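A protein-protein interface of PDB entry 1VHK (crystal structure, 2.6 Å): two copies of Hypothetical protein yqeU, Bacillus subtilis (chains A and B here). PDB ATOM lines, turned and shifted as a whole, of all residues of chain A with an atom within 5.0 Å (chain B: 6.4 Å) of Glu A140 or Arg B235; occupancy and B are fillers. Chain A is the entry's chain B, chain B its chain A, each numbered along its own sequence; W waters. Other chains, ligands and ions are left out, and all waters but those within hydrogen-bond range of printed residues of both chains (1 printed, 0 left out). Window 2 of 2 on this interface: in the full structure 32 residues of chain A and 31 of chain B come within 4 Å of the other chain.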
ATOM      1  N   GLN A 100     -16.688 -21.736  16.532  1.00  0.00           N
ATOM      2  CA  GLN A 100     -17.927 -22.472  16.443  1.00  0.00           C
ATOM      3  C   GLN A 100     -19.054 -21.631  15.866  1.00  0.00           C
ATOM      4  O   GLN A 100     -19.644 -21.958  14.840  1.00  0.00           O
ATOM      5  CB  GLN A 100     -18.326 -23.040  17.811  1.00  0.00           C
ATOM      6  CG  GLN A 100     -19.377 -24.132  17.710  1.00  0.00           C
ATOM      7  CD  GLN A 100     -19.924 -24.544  19.058  1.00  0.00           C
ATOM      8  OE1 GLN A 100     -20.561 -23.736  19.744  1.00  0.00           O
ATOM      9  NE2 GLN A 100     -19.721 -25.779  19.497  1.00  0.00           N
ATOM     10  N   LYS A 101     -19.390 -20.535  16.537  1.00  0.00           N
ATOM     11  CA  LYS A 101     -20.485 -19.703  16.100  1.00  0.00           C
ATOM     12  C   LYS A 101     -20.218 -19.108  14.732  1.00  0.00           C
ATOM     13  O   LYS A 101     -21.159 -19.005  13.914  1.00  0.00           O
ATOM     14  CB  LYS A 101     -20.769 -18.613  17.144  1.00  0.00           C
ATOM     15  CG  LYS A 101     -21.757 -19.081  18.202  1.00  0.00           C
ATOM     16  CD  LYS A 101     -21.192 -20.187  19.074  1.00  0.00           C
ATOM     17  CE  LYS A 101     -22.186 -20.584  20.169  1.00  0.00           C
ATOM     18  NZ  LYS A 101     -22.767 -21.918  19.932  1.00  0.00           N
ATOM     19  N   GLU A 104     -20.822 -21.537  11.954  1.00  0.00           N
ATOM     20  CA  GLU A 104     -22.246 -21.719  11.641  1.00  0.00           C
ATOM     21  C   GLU A 104     -22.813 -20.496  10.948  1.00  0.00           C
ATOM     22  O   GLU A 104     -23.776 -20.570  10.183  1.00  0.00           O
ATOM     23  CB  GLU A 104     -23.007 -22.240  12.821  1.00  0.00           C
ATOM     24  CG  GLU A 104     -23.455 -21.268  13.876  1.00  0.00           C
ATOM     25  CD  GLU A 104     -23.933 -21.961  15.160  1.00  0.00           C
ATOM     26  OE1 GLU A 104     -23.071 -22.437  15.918  1.00  0.00           O
ATOM     27  OE2 GLU A 104     -25.163 -22.030  15.386  1.00  0.00           O
ATOM     28  N   LYS A 136     -10.991 -29.169  15.133  1.00  0.00           N
ATOM     29  CA  LYS A 136     -12.045 -30.108  15.482  1.00  0.00           C
ATOM     30  C   LYS A 136     -13.348 -29.353  15.733  1.00  0.00           C
ATOM     31  O   LYS A 136     -14.387 -29.800  15.265  1.00  0.00           O
ATOM     32  CB  LYS A 136     -11.642 -30.941  16.702  1.00  0.00           C
ATOM     33  CG  LYS A 136     -12.785 -31.778  17.282  1.00  0.00           C
ATOM     34  CD  LYS A 136     -12.355 -32.561  18.497  1.00  0.00           C
ATOM     35  CE  LYS A 136     -12.023 -31.643  19.669  1.00  0.00           C
ATOM     36  NZ  LYS A 136     -11.408 -32.382  20.810  1.00  0.00           N
ATOM     37  N   ILE A 137     -13.278 -28.227  16.438  1.00  0.00           N
ATOM     38  CA  ILE A 137     -14.450 -27.374  16.656  1.00  0.00           C
ATOM     39  C   ILE A 137     -14.999 -26.851  15.334  1.00  0.00           C
ATOM     40  O   ILE A 137     -16.214 -26.863  15.100  1.00  0.00           O
ATOM     41  CB  ILE A 137     -14.152 -26.220  17.620  1.00  0.00           C
ATOM     42  CG1 ILE A 137     -13.967 -26.789  19.056  1.00  0.00           C
ATOM     43  CG2 ILE A 137     -15.240 -25.176  17.665  1.00  0.00           C
ATOM     44  CD1 ILE A 137     -13.247 -25.807  19.953  1.00  0.00           C
ATOM     45  N   ALA A 138     -14.153 -26.461  14.405  1.00  0.00           N
ATOM     46  CA  ALA A 138     -14.588 -26.018  13.084  1.00  0.00           C
ATOM     47  C   ALA A 138     -15.368 -27.117  12.365  1.00  0.00           C
ATOM     48  O   ALA A 138     -16.562 -26.993  12.080  1.00  0.00           O
ATOM     49  CB  ALA A 138     -13.388 -25.617  12.262  1.00  0.00           C
ATOM     50  N   LYS A 139     -14.738 -28.255  12.133  1.00  0.00           N
ATOM     51  CA  LYS A 139     -15.352 -29.371  11.452  1.00  0.00           C
ATOM     52  C   LYS A 139     -16.709 -29.776  12.014  1.00  0.00           C
ATOM     53  O   LYS A 139     -17.653 -30.027  11.229  1.00  0.00           O
ATOM     54  CB  LYS A 139     -14.410 -30.566  11.426  1.00  0.00           C
ATOM     55  CG  LYS A 139     -14.972 -31.782  10.698  1.00  0.00           C
ATOM     56  CD  LYS A 139     -13.889 -32.861  10.614  1.00  0.00           C
ATOM     57  CE  LYS A 139     -14.493 -34.243  10.458  1.00  0.00           C
ATOM     58  NZ  LYS A 139     -13.478 -35.311  10.730  1.00  0.00           N
ATOM     59  N   GLU A 140     -16.824 -29.885  13.338  1.00  0.00           N
ATOM     60  CA  GLU A 140     -18.090 -30.288  13.942  1.00  0.00           C
ATOM     61  C   GLU A 140     -19.153 -29.213  13.735  1.00  0.00           C
ATOM     62  O   GLU A 140     -20.335 -29.506  13.562  1.00  0.00           O
ATOM     63  CB  GLU A 140     -17.903 -30.572  15.431  1.00  0.00           C
ATOM     64  CG  GLU A 140     -19.025 -31.307  16.097  1.00  0.00           C
ATOM     65  CD  GLU A 140     -20.191 -30.472  16.563  1.00  0.00           C
ATOM     66  OE1 GLU A 140     -20.073 -29.224  16.674  1.00  0.00           O
ATOM     67  OE2 GLU A 140     -21.257 -31.093  16.848  1.00  0.00           O
ATOM     68  N   ALA A 141     -18.720 -27.945  13.832  1.00  0.00           N
ATOM     69  CA  ALA A 141     -19.603 -26.802  13.616  1.00  0.00           C
ATOM     70  C   ALA A 141     -20.040 -26.808  12.143  1.00  0.00           C
ATOM     71  O   ALA A 141     -21.201 -26.641  11.837  1.00  0.00           O
ATOM     72  CB  ALA A 141     -18.922 -25.502  13.971  1.00  0.00           C
ATOM     73  N   ALA A 142     -19.105 -27.137  11.245  1.00  0.00           N
ATOM     74  CA  ALA A 142     -19.461 -27.253   9.849  1.00  0.00           C
ATOM     75  C   ALA A 142     -20.496 -28.368   9.671  1.00  0.00           C
ATOM     76  O   ALA A 142     -21.555 -28.161   9.071  1.00  0.00           O
ATOM     77  CB  ALA A 142     -18.245 -27.478   8.990  1.00  0.00           C
ATOM     78  N   GLU A 143     -20.225 -29.529  10.254  1.00  0.00           N
ATOM     79  CA  GLU A 143     -21.115 -30.662  10.154  1.00  0.00           C
ATOM     80  C   GLU A 143     -22.557 -30.309  10.479  1.00  0.00           C
ATOM     81  O   GLU A 143     -23.409 -30.367   9.594  1.00  0.00           O
ATOM     82  CB  GLU A 143     -20.633 -31.835  11.004  1.00  0.00           C
ATOM     83  CG  GLU A 143     -19.514 -32.643  10.399  1.00  0.00           C
ATOM     84  CD  GLU A 143     -18.818 -33.574  11.365  1.00  0.00           C
ATOM     85  OE1 GLU A 143     -18.130 -34.510  10.887  1.00  0.00           O
ATOM     86  OE2 GLU A 143     -18.925 -33.421  12.609  1.00  0.00           O
ATOM     87  N   GLN A 144     -22.823 -29.904  11.697  1.00  0.00           N
ATOM     88  CA  GLN A 144     -24.134 -29.556  12.186  1.00  0.00           C
ATOM     89  C   GLN A 144     -24.841 -28.423  11.478  1.00  0.00           C
ATOM     90  O   GLN A 144     -26.078 -28.391  11.509  1.00  0.00           O
ATOM     91  CB  GLN A 144     -24.030 -29.196  13.693  1.00  0.00           C
ATOM     92  CG  GLN A 144     -23.504 -30.369  14.530  1.00  0.00           C
ATOM     93  CD  GLN A 144     -24.549 -31.490  14.573  1.00  0.00           C
ATOM     94  OE1 GLN A 144     -24.291 -32.608  14.128  1.00  0.00           O
ATOM     95  NE2 GLN A 144     -25.725 -31.140  15.090  1.00  0.00           N
ATOM     96  N   ILE B 233     -27.933 -23.944   9.113  1.00  0.00           N
ATOM     97  CA  ILE B 233     -28.647 -24.306  10.341  1.00  0.00           C
ATOM     98  C   ILE B 233     -27.918 -23.825  11.587  1.00  0.00           C
ATOM     99  O   ILE B 233     -26.741 -24.075  11.851  1.00  0.00           O
ATOM    100  CB  ILE B 233     -28.944 -25.807  10.376  1.00  0.00           C
ATOM    101  CG1 ILE B 233     -29.840 -26.169   9.160  1.00  0.00           C
ATOM    102  CG2 ILE B 233     -29.577 -26.252  11.674  1.00  0.00           C
ATOM    103  CD1 ILE B 233     -31.151 -25.376   9.104  1.00  0.00           C
ATOM    104  N   LEU B 234     -28.626 -23.042  12.401  1.00  0.00           N
ATOM    105  CA  LEU B 234     -28.157 -22.348  13.564  1.00  0.00           C
ATOM    106  C   LEU B 234     -28.544 -22.968  14.895  1.00  0.00           C
ATOM    107  O   LEU B 234     -29.646 -23.437  15.097  1.00  0.00           O
ATOM    108  CB  LEU B 234     -28.678 -20.898  13.488  1.00  0.00           C
ATOM    109  CG  LEU B 234     -27.916 -19.849  12.694  1.00  0.00           C
ATOM    110  CD1 LEU B 234     -26.851 -20.398  11.780  1.00  0.00           C
ATOM    111  CD2 LEU B 234     -28.884 -18.980  11.893  1.00  0.00           C
ATOM    112  N   ARG B 235     -27.622 -22.959  15.865  1.00  0.00           N
ATOM    113  CA  ARG B 235     -27.925 -23.491  17.189  1.00  0.00           C
ATOM    114  C   ARG B 235     -28.858 -22.545  17.926  1.00  0.00           C
ATOM    115  O   ARG B 235     -28.989 -21.365  17.592  1.00  0.00           O
ATOM    116  CB  ARG B 235     -26.633 -23.768  17.973  1.00  0.00           C
ATOM    117  CG  ARG B 235     -25.737 -24.793  17.270  1.00  0.00           C
ATOM    118  CD  ARG B 235     -24.330 -24.815  17.804  1.00  0.00           C
ATOM    119  NE  ARG B 235     -23.388 -25.515  16.918  1.00  0.00           N
ATOM    120  CZ  ARG B 235     -22.501 -26.406  17.335  1.00  0.00           C
ATOM    121  NH1 ARG B 235     -21.677 -26.994  16.478  1.00  0.00           N
ATOM    122  NH2 ARG B 235     -22.420 -26.748  18.632  1.00  0.00           N
ATOM    123  N   THR B 236     -29.544 -23.036  18.972  1.00  0.00           N
ATOM    124  CA  THR B 236     -30.485 -22.251  19.705  1.00  0.00           C
ATOM    125  C   THR B 236     -29.941 -20.972  20.304  1.00  0.00           C
ATOM    126  O   THR B 236     -30.769 -20.070  20.518  1.00  0.00           O
ATOM    127  CB  THR B 236     -31.190 -22.993  20.874  1.00  0.00           C
ATOM    128  OG1 THR B 236     -30.267 -23.779  21.616  1.00  0.00           O
ATOM    129  CG2 THR B 236     -32.245 -23.821  20.220  1.00  0.00           C
ATOM    130  N   GLU B 237     -28.687 -21.025  20.718  1.00  0.00           N
ATOM    131  CA  GLU B 237     -27.989 -19.897  21.285  1.00  0.00           C
ATOM    132  C   GLU B 237     -27.507 -18.957  20.176  1.00  0.00           C
ATOM    133  O   GLU B 237     -27.419 -17.744  20.406  1.00  0.00           O
ATOM    134  CB  GLU B 237     -26.872 -20.331  22.224  1.00  0.00           C
ATOM    135  CG  GLU B 237     -25.730 -21.099  21.646  1.00  0.00           C
ATOM    136  CD  GLU B 237     -25.918 -22.565  21.396  1.00  0.00           C
ATOM    137  OE1 GLU B 237     -27.050 -23.045  21.152  1.00  0.00           O
ATOM    138  OE2 GLU B 237     -24.907 -23.324  21.417  1.00  0.00           O
ATOM    139  N   THR B 238     -27.448 -19.439  18.939  1.00  0.00           N
ATOM    140  CA  THR B 238     -26.979 -18.681  17.787  1.00  0.00           C
ATOM    141  C   THR B 238     -28.059 -17.934  17.036  1.00  0.00           C
ATOM    142  O   THR B 238     -27.886 -16.723  16.767  1.00  0.00           O
ATOM    143  CB  THR B 238     -26.178 -19.549  16.797  1.00  0.00           C
ATOM    144  OG1 THR B 238     -25.300 -20.433  17.512  1.00  0.00           O
ATOM    145  CG2 THR B 238     -25.333 -18.691  15.870  1.00  0.00           C
ATOM    146  N   ALA B 239     -29.216 -18.515  16.800  1.00  0.00           N
ATOM    147  CA  ALA B 239     -30.329 -17.935  16.073  1.00  0.00           C
ATOM    148  C   ALA B 239     -30.739 -16.536  16.470  1.00  0.00           C
ATOM    149  O   ALA B 239     -30.860 -15.653  15.618  1.00  0.00           O
ATOM    150  CB  ALA B 239     -31.563 -18.840  16.127  1.00  0.00           C
ATOM    151  N   PRO B 240     -31.006 -16.271  17.741  1.00  0.00           N
ATOM    152  CA  PRO B 240     -31.390 -14.959  18.211  1.00  0.00           C
ATOM    153  C   PRO B 240     -30.307 -13.891  18.034  1.00  0.00           C
ATOM    154  O   PRO B 240     -30.609 -12.692  17.975  1.00  0.00           O
ATOM    155  CB  PRO B 240     -31.684 -15.132  19.677  1.00  0.00           C
ATOM    156  CG  PRO B 240     -31.577 -16.549  19.996  1.00  0.00           C
ATOM    157  CD  PRO B 240     -31.037 -17.280  18.811  1.00  0.00           C
HETATM  158  O   HOH W   1     -22.702 -25.962  14.101  1.00  0.00           O
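Printed residues of chain B within 4 Å of Glu A140: Arg B235 (2.8 Å). Arg B235 touches just these residues of chain A: Gln A100 (3.0 Å), Lys A101 (3.9 Å), Glu A104 (2.7 Å), Glu A140 (2.8 Å) and Ala A141 (3.5 Å). Printed residues of chain A within 4 Å of Leu B234: Glu A104 (3.5 Å). Printed residues of chain A within 4 Å of Thr B238: Lys A101 (3.8 Å) and Glu A104 (2.7 Å). Printed residues of chain B within 4 Å of Ala A141: Arg B235 (3.5 Å). Of the printed residues of chain A, Glu B237 touches Lys A101 (3.0 Å). Of the printed residues of chain B, Lys A101 touches Arg B235 (3.9 Å), Glu B237 (3.0 Å) and Thr B238 (3.8 Å). Ala B239 touches none of the printed residues of chain A. The nearest printed residue of chain B that does not touch Glu A140 is Ile B233 (8.6 Å). The nearest residue of chain A that does not touch Arg B235 is Gln A144 (4.3 Å). The nearest printed residue of chain B that does not touch Gln A100 is Glu B237 (4.7 Å).
The guanidinium group (NE) of Arg B235 is in salt-bridge range of the side-chain carboxylate (OE1) of Glu A104. The guanidinium group of Arg B235 lies close to the side-chain amide nitrogen of Gln A100 (3.0 Å). NH1 of Arg B235 is in salt-bridge range of OE1 of Glu A140 (2.8 Å). The side-chain hydroxyl (OG1) of Thr B238 is in hydrogen-bond range of the side-chain carboxylate (OE2) of Glu A104 (2.7 Å). OE2 of Glu B237 lies within salt-bridge range of NZ of Lys A101.
Of the 12 printed residues of chain A, 5 touch a printed residue of chain B. Along chain A the printed residues that touch a printed residue of chain B span positions 100 to 141. Printed residues of chain B that touch a printed residue of chain A: Leu B234, Arg B235, Glu B237 and Thr B238. Hydrophobic or aromatic side chains of chain B that line the printed part of chain A: Leu B234. Among the printed residues, Asp or Glu carboxylates within 4 Å of a Lys or Arg side-chain nitrogen of the other chain: Lys A101 with Glu B237, Glu A104 with Arg B235 and Glu A140 with Arg B235.
No position is printed for both chains. Of the 9 pairs that touch across the chains among the printed residues, none has its exchanged pair printed and touching as well.
The side-chain amide oxygen (OE1) of Gln A100 sits at hydrogen-bond distance from the side-chain amino group (NZ) of Lys A101 (2.9 Å). OG1 of Thr B236 sits at hydrogen-bond distance from OE1 of Glu B237, 3.3 Å away.
Water W1 bridges the guanidinium group of Arg B235 (2.8 Å) and the backbone carbonyl oxygen of Ala A141 (2.8 Å).
Among the printed residues, merely in contact across the chains: Glu A104 with Leu B234, Ala A141 with Arg B235, Lys A101 with Thr B238 and Lys A101 with Arg B235.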
